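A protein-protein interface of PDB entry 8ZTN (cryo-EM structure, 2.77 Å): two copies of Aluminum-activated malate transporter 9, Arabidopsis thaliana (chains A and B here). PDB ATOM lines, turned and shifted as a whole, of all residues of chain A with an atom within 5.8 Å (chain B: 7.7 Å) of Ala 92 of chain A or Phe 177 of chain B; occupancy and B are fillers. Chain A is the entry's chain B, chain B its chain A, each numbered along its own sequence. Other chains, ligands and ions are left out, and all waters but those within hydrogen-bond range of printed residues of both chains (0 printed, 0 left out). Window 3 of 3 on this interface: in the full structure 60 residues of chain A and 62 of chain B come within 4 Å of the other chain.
No position is printed for both chains.
Of the 12 pairs that touch across the chains among the printed residues, none has its exchanged pair printed and touching as well.
O of Gly 180 of chain B is in hydrogen-bond range of OG1 of Thr 184 of chain B.
OG1 of Thr 99 of chain A is in hydrogen-bond range of O of Gly 95 of chain A, at 3.4 Å.
Printed residues of chain B within 4 Å of Ile 88 of chain A: Phe 181 (3.9 Å) and Phe 185 (3.9 Å).
Val 89 of chain A touches none of the printed residues of chain B.
Of chain B, only Phe 177 (3.9 Å) and Phe 181 (3.9 Å) come within 4 Å of Ala 92 of chain A.
Printed residues of chain B within 4 Å of Gly 95 of chain A: Phe 177.
Printed residues of chain B within 4 Å of Thr 99 of chain A: Thr 173 (3.5 Å) and Phe 177 (3.5 Å).
Phe 177 of chain B touches four residues of chain A.
Leu 182 of chain B touches none of the printed residues of chain A.
Of the printed residues of chain A, Thr 184 of chain B touches Ser 91 (3.8 Å) and Ile 94 (3.3 Å).
The nearest residue of chain A that does not touch Phe 177 of chain B is Ser 91 of chain A (5.5 Å).
The nearest printed residue of chain A that does not touch Thr 184 of chain B is Phe 90 of chain A (4.1 Å).
Among the printed residues, merely in contact across the chains: Ile 88 of chain A with Phe 181 of chain B, Ile 88 of chain A with Phe 185 of chain B, Ser 91 of chain A with Phe 181 of chain B, Ser 91 of chain A with Thr 184 of chain B, Ser 91 of chain A with Phe 185 of chain B, Ala 92 of chain A with Phe 177 of chain B, Ala 92 of chain A with Phe 181 of chain B, Ile 94 of chain A with Thr 184 of chain B, Gly 95 of chain A with Phe 177 of chain B, Leu 96 of chain A with Phe 177 of chain B, Thr 99 of chain A with Thr 173 of chain B and Thr 99 of chain A with Phe 177 of chain B.
Of the 11 printed residues of chain A, 7 touch a printed residue of chain B.
Printed residues of chain A that touch a printed residue of chain B: Ile 88, Ser 91, Ala 92, Ile 94, Gly 95, Leu 96 and Thr 99.
Of the 17 printed residues of chain B, 5 touch a printed residue of chain A.
Among the printed residues, 12 pairs touch across the chains.
Among the printed residues, no Asp or Glu carboxylate lies within 4 Å of a Lys or Arg side-chain nitrogen of the other chain.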
ATOM      1  N   ILE A  88      13.134  26.280   0.660  1.00  0.00           N
ATOM      2  CA  ILE A  88      13.630  24.986   0.203  1.00  0.00           C
ATOM      3  C   ILE A  88      14.486  24.300   1.255  1.00  0.00           C
ATOM      4  O   ILE A  88      14.745  23.091   1.140  1.00  0.00           O
ATOM      5  CB  ILE A  88      14.421  25.134  -1.117  1.00  0.00           C
ATOM      6  CG1 ILE A  88      13.472  25.436  -2.276  1.00  0.00           C
ATOM      7  CG2 ILE A  88      15.226  23.882  -1.420  1.00  0.00           C
ATOM      8  CD1 ILE A  88      14.057  26.364  -3.312  1.00  0.00           C
ATOM      9  N   VAL A  89      14.904  25.019   2.292  1.00  0.00           N
ATOM     10  CA  VAL A  89      15.682  24.425   3.370  1.00  0.00           C
ATOM     11  C   VAL A  89      14.776  23.918   4.489  1.00  0.00           C
ATOM     12  O   VAL A  89      15.081  22.899   5.117  1.00  0.00           O
ATOM     13  CB  VAL A  89      16.709  25.440   3.901  1.00  0.00           C
ATOM     14  CG1 VAL A  89      17.518  24.840   5.041  1.00  0.00           C
ATOM     15  CG2 VAL A  89      17.622  25.902   2.780  1.00  0.00           C
ATOM     16  N   PHE A  90      13.662  24.607   4.744  1.00  0.00           N
ATOM     17  CA  PHE A  90      12.706  24.158   5.750  1.00  0.00           C
ATOM     18  C   PHE A  90      12.110  22.800   5.385  1.00  0.00           C
ATOM     19  O   PHE A  90      11.988  21.909   6.240  1.00  0.00           O
ATOM     20  CB  PHE A  90      11.612  25.219   5.899  1.00  0.00           C
ATOM     21  CG  PHE A  90      10.623  24.941   6.992  1.00  0.00           C
ATOM     22  CD1 PHE A  90      11.007  24.990   8.320  1.00  0.00           C
ATOM     23  CD2 PHE A  90       9.303  24.654   6.694  1.00  0.00           C
ATOM     24  CE1 PHE A  90      10.098  24.744   9.324  1.00  0.00           C
ATOM     25  CE2 PHE A  90       8.392  24.407   7.696  1.00  0.00           C
ATOM     26  CZ  PHE A  90       8.790  24.452   9.012  1.00  0.00           C
ATOM     27  N   SER A  91      11.750  22.617   4.111  1.00  0.00           N
ATOM     28  CA  SER A  91      11.182  21.348   3.668  1.00  0.00           C
ATOM     29  C   SER A  91      12.191  20.212   3.782  1.00  0.00           C
ATOM     30  O   SER A  91      11.839  19.094   4.181  1.00  0.00           O
ATOM     31  CB  SER A  91      10.685  21.478   2.230  1.00  0.00           C
ATOM     32  OG  SER A  91       9.883  22.634   2.073  1.00  0.00           O
ATOM     33  N   ALA A  92      13.461  20.488   3.482  1.00  0.00           N
ATOM     34  CA  ALA A  92      14.474  19.445   3.593  1.00  0.00           C
ATOM     35  C   ALA A  92      14.810  19.153   5.048  1.00  0.00           C
ATOM     36  O   ALA A  92      15.155  18.017   5.385  1.00  0.00           O
ATOM     37  CB  ALA A  92      15.728  19.843   2.818  1.00  0.00           C
ATOM     38  N   LYS A  93      14.674  20.145   5.928  1.00  0.00           N
ATOM     39  CA  LYS A  93      14.876  19.895   7.350  1.00  0.00           C
ATOM     40  C   LYS A  93      13.769  19.009   7.912  1.00  0.00           C
ATOM     41  O   LYS A  93      14.031  18.100   8.712  1.00  0.00           O
ATOM     42  CB  LYS A  93      14.944  21.224   8.099  1.00  0.00           C
ATOM     43  CG  LYS A  93      16.228  21.998   7.859  1.00  0.00           C
ATOM     44  CD  LYS A  93      16.595  22.846   9.058  1.00  0.00           C
ATOM     45  CE  LYS A  93      15.503  23.841   9.385  1.00  0.00           C
ATOM     46  NZ  LYS A  93      16.024  24.983  10.179  1.00  0.00           N
ATOM     47  N   ILE A  94      12.528  19.241   7.479  1.00  0.00           N
ATOM     48  CA  ILE A  94      11.439  18.362   7.899  1.00  0.00           C
ATOM     49  C   ILE A  94      11.646  16.955   7.350  1.00  0.00           C
ATOM     50  O   ILE A  94      11.444  15.959   8.061  1.00  0.00           O
ATOM     51  CB  ILE A  94      10.079  18.945   7.477  1.00  0.00           C
ATOM     52  CG1 ILE A  94       9.921  20.366   8.016  1.00  0.00           C
ATOM     53  CG2 ILE A  94       8.943  18.058   7.955  1.00  0.00           C
ATOM     54  CD1 ILE A  94       8.586  20.988   7.698  1.00  0.00           C
ATOM     55  N   GLY A  95      12.059  16.844   6.086  1.00  0.00           N
ATOM     56  CA  GLY A  95      12.339  15.528   5.534  1.00  0.00           C
ATOM     57  C   GLY A  95      13.447  14.806   6.278  1.00  0.00           C
ATOM     58  O   GLY A  95      13.372  13.594   6.498  1.00  0.00           O
ATOM     59  N   LEU A  96      14.476  15.543   6.705  1.00  0.00           N
ATOM     60  CA  LEU A  96      15.580  14.930   7.436  1.00  0.00           C
ATOM     61  C   LEU A  96      15.144  14.446   8.815  1.00  0.00           C
ATOM     62  O   LEU A  96      15.506  13.339   9.233  1.00  0.00           O
ATOM     63  CB  LEU A  96      16.736  15.922   7.558  1.00  0.00           C
ATOM     64  CG  LEU A  96      17.940  15.494   8.398  1.00  0.00           C
ATOM     65  CD1 LEU A  96      18.805  14.505   7.634  1.00  0.00           C
ATOM     66  CD2 LEU A  96      18.751  16.706   8.826  1.00  0.00           C
ATOM     67  N   ALA A  97      14.350  15.247   9.530  1.00  0.00           N
ATOM     68  CA  ALA A  97      13.864  14.799  10.833  1.00  0.00           C
ATOM     69  C   ALA A  97      12.986  13.562  10.690  1.00  0.00           C
ATOM     70  O   ALA A  97      13.097  12.603  11.476  1.00  0.00           O
ATOM     71  CB  ALA A  97      13.102  15.927  11.527  1.00  0.00           C
ATOM     72  N   THR A  99      13.042  11.306   8.267  1.00  0.00           N
ATOM     73  CA  THR A  99      13.883  10.167   7.913  1.00  0.00           C
ATOM     74  C   THR A  99      14.661   9.644   9.113  1.00  0.00           C
ATOM     75  O   THR A  99      14.843   8.428   9.250  1.00  0.00           O
ATOM     76  CB  THR A  99      14.841  10.557   6.787  1.00  0.00           C
ATOM     77  OG1 THR A  99      14.161  10.475   5.530  1.00  0.00           O
ATOM     78  CG2 THR A  99      16.043   9.630   6.764  1.00  0.00           C
ATOM     79  N   PHE B 171      14.129   1.761   0.683  1.00  0.00           N
ATOM     80  CA  PHE B 171      13.213   2.423  -0.240  1.00  0.00           C
ATOM     81  C   PHE B 171      12.028   3.028   0.506  1.00  0.00           C
ATOM     82  O   PHE B 171      11.582   4.142   0.189  1.00  0.00           O
ATOM     83  CB  PHE B 171      12.754   1.421  -1.303  1.00  0.00           C
ATOM     84  CG  PHE B 171      11.582   1.880  -2.123  1.00  0.00           C
ATOM     85  CD1 PHE B 171      11.772   2.681  -3.236  1.00  0.00           C
ATOM     86  CD2 PHE B 171      10.296   1.487  -1.800  1.00  0.00           C
ATOM     87  CE1 PHE B 171      10.699   3.095  -3.999  1.00  0.00           C
ATOM     88  CE2 PHE B 171       9.219   1.899  -2.560  1.00  0.00           C
ATOM     89  CZ  PHE B 171       9.421   2.703  -3.661  1.00  0.00           C
ATOM     90  N   CYS B 172      11.530   2.329   1.528  1.00  0.00           N
ATOM     91  CA  CYS B 172      10.391   2.850   2.274  1.00  0.00           C
ATOM     92  C   CYS B 172      10.771   4.087   3.082  1.00  0.00           C
ATOM     93  O   CYS B 172       9.975   5.026   3.193  1.00  0.00           O
ATOM     94  CB  CYS B 172       9.820   1.766   3.187  1.00  0.00           C
ATOM     95  SG  CYS B 172       8.714   0.607   2.351  1.00  0.00           S
ATOM     96  N   THR B 173      11.979   4.111   3.652  1.00  0.00           N
ATOM     97  CA  THR B 173      12.448   5.290   4.367  1.00  0.00           C
ATOM     98  C   THR B 173      12.916   6.398   3.434  1.00  0.00           C
ATOM     99  O   THR B 173      13.056   7.543   3.877  1.00  0.00           O
ATOM    100  CB  THR B 173      13.586   4.912   5.319  1.00  0.00           C
ATOM    101  OG1 THR B 173      13.805   5.976   6.252  1.00  0.00           O
ATOM    102  CG2 THR B 173      14.866   4.657   4.543  1.00  0.00           C
ATOM    103  N   LEU B 174      13.162   6.090   2.161  1.00  0.00           N
ATOM    104  CA  LEU B 174      13.523   7.112   1.192  1.00  0.00           C
ATOM    105  C   LEU B 174      12.315   7.698   0.480  1.00  0.00           C
ATOM    106  O   LEU B 174      12.446   8.729  -0.187  1.00  0.00           O
ATOM    107  CB  LEU B 174      14.496   6.537   0.158  1.00  0.00           C
ATOM    108  CG  LEU B 174      15.199   7.542  -0.753  1.00  0.00           C
ATOM    109  CD1 LEU B 174      16.686   7.246  -0.822  1.00  0.00           C
ATOM    110  CD2 LEU B 174      14.581   7.532  -2.142  1.00  0.00           C
ATOM    111  N   SER B 175      11.147   7.067   0.608  1.00  0.00           N
ATOM    112  CA  SER B 175       9.935   7.655   0.044  1.00  0.00           C
ATOM    113  C   SER B 175       9.309   8.663   1.001  1.00  0.00           C
ATOM    114  O   SER B 175       8.676   9.631   0.558  1.00  0.00           O
ATOM    115  CB  SER B 175       8.924   6.561  -0.297  1.00  0.00           C
ATOM    116  OG  SER B 175       9.442   5.662  -1.261  1.00  0.00           O
ATOM    117  N   ILE B 176       9.505   8.460   2.305  1.00  0.00           N
ATOM    118  CA  ILE B 176       9.003   9.397   3.306  1.00  0.00           C
ATOM    119  C   ILE B 176       9.665  10.758   3.146  1.00  0.00           C
ATOM    120  O   ILE B 176       9.006  11.797   3.257  1.00  0.00           O
ATOM    121  CB  ILE B 176       9.213   8.824   4.719  1.00  0.00           C
ATOM    122  CG1 ILE B 176       8.347   7.578   4.915  1.00  0.00           C
ATOM    123  CG2 ILE B 176       8.912   9.870   5.779  1.00  0.00           C
ATOM    124  CD1 ILE B 176       8.674   6.799   6.160  1.00  0.00           C
ATOM    125  N   PHE B 177      10.972  10.776   2.874  1.00  0.00           N
ATOM    126  CA  PHE B 177      11.671  12.043   2.677  1.00  0.00           C
ATOM    127  C   PHE B 177      11.081  12.818   1.505  1.00  0.00           C
ATOM    128  O   PHE B 177      10.775  14.012   1.624  1.00  0.00           O
ATOM    129  CB  PHE B 177      13.163  11.782   2.454  1.00  0.00           C
ATOM    130  CG  PHE B 177      13.963  13.022   2.168  1.00  0.00           C
ATOM    131  CD1 PHE B 177      14.440  13.811   3.199  1.00  0.00           C
ATOM    132  CD2 PHE B 177      14.235  13.400   0.865  1.00  0.00           C
ATOM    133  CE1 PHE B 177      15.173  14.953   2.933  1.00  0.00           C
ATOM    134  CE2 PHE B 177      14.963  14.539   0.595  1.00  0.00           C
ATOM    135  CZ  PHE B 177      15.432  15.316   1.631  1.00  0.00           C
ATOM    136  N   CYS B 178      10.911  12.151   0.363  1.00  0.00           N
ATOM    137  CA  CYS B 178      10.392  12.825  -0.823  1.00  0.00           C
ATOM    138  C   CYS B 178       8.971  13.324  -0.602  1.00  0.00           C
ATOM    139  O   CYS B 178       8.634  14.456  -0.979  1.00  0.00           O
ATOM    140  CB  CYS B 178      10.449  11.883  -2.025  1.00  0.00           C
ATOM    141  SG  CYS B 178      12.092  11.210  -2.369  1.00  0.00           S
ATOM    142  N   ILE B 179       8.120  12.502   0.018  1.00  0.00           N
ATOM    143  CA  ILE B 179       6.736  12.917   0.211  1.00  0.00           C
ATOM    144  C   ILE B 179       6.651  14.060   1.215  1.00  0.00           C
ATOM    145  O   ILE B 179       5.867  14.999   1.033  1.00  0.00           O
ATOM    146  CB  ILE B 179       5.870  11.718   0.639  1.00  0.00           C
ATOM    147  CG1 ILE B 179       5.837  10.669  -0.470  1.00  0.00           C
ATOM    148  CG2 ILE B 179       4.465  12.173   0.982  1.00  0.00           C
ATOM    149  CD1 ILE B 179       4.978  11.057  -1.649  1.00  0.00           C
ATOM    150  N   GLY B 180       7.472  14.027   2.267  1.00  0.00           N
ATOM    151  CA  GLY B 180       7.477  15.130   3.212  1.00  0.00           C
ATOM    152  C   GLY B 180       7.965  16.419   2.584  1.00  0.00           C
ATOM    153  O   GLY B 180       7.406  17.491   2.832  1.00  0.00           O
ATOM    154  N   PHE B 181       8.969  16.326   1.710  1.00  0.00           N
ATOM    155  CA  PHE B 181       9.479  17.523   1.056  1.00  0.00           C
ATOM    156  C   PHE B 181       8.427  18.124   0.134  1.00  0.00           C
ATOM    157  O   PHE B 181       8.193  19.339   0.155  1.00  0.00           O
ATOM    158  CB  PHE B 181      10.754  17.195   0.280  1.00  0.00           C
ATOM    159  CG  PHE B 181      11.286  18.343  -0.532  1.00  0.00           C
ATOM    160  CD1 PHE B 181      12.149  19.265   0.031  1.00  0.00           C
ATOM    161  CD2 PHE B 181      10.919  18.505  -1.857  1.00  0.00           C
ATOM    162  CE1 PHE B 181      12.636  20.324  -0.710  1.00  0.00           C
ATOM    163  CE2 PHE B 181      11.403  19.561  -2.600  1.00  0.00           C
ATOM    164  CZ  PHE B 181      12.263  20.471  -2.026  1.00  0.00           C
ATOM    165  N   LEU B 182       7.755  17.285  -0.659  1.00  0.00           N
ATOM    166  CA  LEU B 182       6.774  17.819  -1.598  1.00  0.00           C
ATOM    167  C   LEU B 182       5.543  18.355  -0.874  1.00  0.00           C
ATOM    168  O   LEU B 182       4.998  19.400  -1.255  1.00  0.00           O
ATOM    169  CB  LEU B 182       6.380  16.745  -2.610  1.00  0.00           C
ATOM    170  CG  LEU B 182       7.486  16.307  -3.569  1.00  0.00           C
ATOM    171  CD1 LEU B 182       7.179  14.943  -4.159  1.00  0.00           C
ATOM    172  CD2 LEU B 182       7.671  17.336  -4.666  1.00  0.00           C
ATOM    173  N   ALA B 183       5.129  17.696   0.213  1.00  0.00           N
ATOM    174  CA  ALA B 183       3.962  18.151   0.957  1.00  0.00           C
ATOM    175  C   ALA B 183       4.249  19.380   1.801  1.00  0.00           C
ATOM    176  O   ALA B 183       3.315  20.115   2.132  1.00  0.00           O
ATOM    177  CB  ALA B 183       3.429  17.024   1.844  1.00  0.00           C
ATOM    178  N   THR B 184       5.512  19.630   2.148  1.00  0.00           N
ATOM    179  CA  THR B 184       5.854  20.860   2.843  1.00  0.00           C
ATOM    180  C   THR B 184       6.123  22.006   1.883  1.00  0.00           C
ATOM    181  O   THR B 184       5.960  23.169   2.267  1.00  0.00           O
ATOM    182  CB  THR B 184       7.082  20.655   3.734  1.00  0.00           C
ATOM    183  OG1 THR B 184       6.981  19.395   4.406  1.00  0.00           O
ATOM    184  CG2 THR B 184       7.187  21.771   4.760  1.00  0.00           C
ATOM    185  N   PHE B 185       6.521  21.708   0.646  1.00  0.00           N
ATOM    186  CA  PHE B 185       6.738  22.769  -0.325  1.00  0.00           C
ATOM    187  C   PHE B 185       5.440  23.213  -0.983  1.00  0.00           C
ATOM    188  O   PHE B 185       5.320  24.379  -1.374  1.00  0.00           O
ATOM    189  CB  PHE B 185       7.737  22.318  -1.391  1.00  0.00           C
ATOM    190  CG  PHE B 185       8.296  23.443  -2.210  1.00  0.00           C
ATOM    191  CD1 PHE B 185       9.077  24.422  -1.624  1.00  0.00           C
ATOM    192  CD2 PHE B 185       8.033  23.526  -3.564  1.00  0.00           C
ATOM    193  CE1 PHE B 185       9.589  25.461  -2.374  1.00  0.00           C
ATOM    194  CE2 PHE B 185       8.543  24.563  -4.319  1.00  0.00           C
ATOM    195  CZ  PHE B 185       9.322  25.531  -3.723  1.00  0.00           C
ATOM    196  N   LEU B 203      -0.184  14.166   5.014  1.00  0.00           N
ATOM    197  CA  LEU B 203       1.086  13.675   5.544  1.00  0.00           C
ATOM    198  C   LEU B 203       0.864  12.632   6.636  1.00  0.00           C
ATOM    199  O   LEU B 203       1.534  11.587   6.656  1.00  0.00           O
ATOM    200  CB  LEU B 203       1.921  14.838   6.076  1.00  0.00           C
ATOM    201  CG  LEU B 203       3.435  14.756   5.870  1.00  0.00           C
ATOM    202  CD1 LEU B 203       3.778  14.120   4.535  1.00  0.00           C
ATOM    203  CD2 LEU B 203       4.067  16.130   5.988  1.00  0.00           C
ATOM    204  N   TYR B 206      -0.318   9.244   5.036  1.00  0.00           N
ATOM    205  CA  TYR B 206       0.754   8.537   4.343  1.00  0.00           C
ATOM    206  C   TYR B 206       1.706   7.887   5.339  1.00  0.00           C
ATOM    207  O   TYR B 206       2.029   6.695   5.228  1.00  0.00           O
ATOM    208  CB  TYR B 206       1.511   9.489   3.420  1.00  0.00           C
ATOM    209  CG  TYR B 206       2.553   8.798   2.569  1.00  0.00           C
ATOM    210  CD1 TYR B 206       2.203   8.185   1.375  1.00  0.00           C
ATOM    211  CD2 TYR B 206       3.883   8.743   2.967  1.00  0.00           C
ATOM    212  CE1 TYR B 206       3.145   7.548   0.596  1.00  0.00           C
ATOM    213  CE2 TYR B 206       4.833   8.107   2.196  1.00  0.00           C
ATOM    214  CZ  TYR B 206       4.457   7.511   1.011  1.00  0.00           C
ATOM    215  OH  TYR B 206       5.395   6.874   0.232  1.00  0.00           O
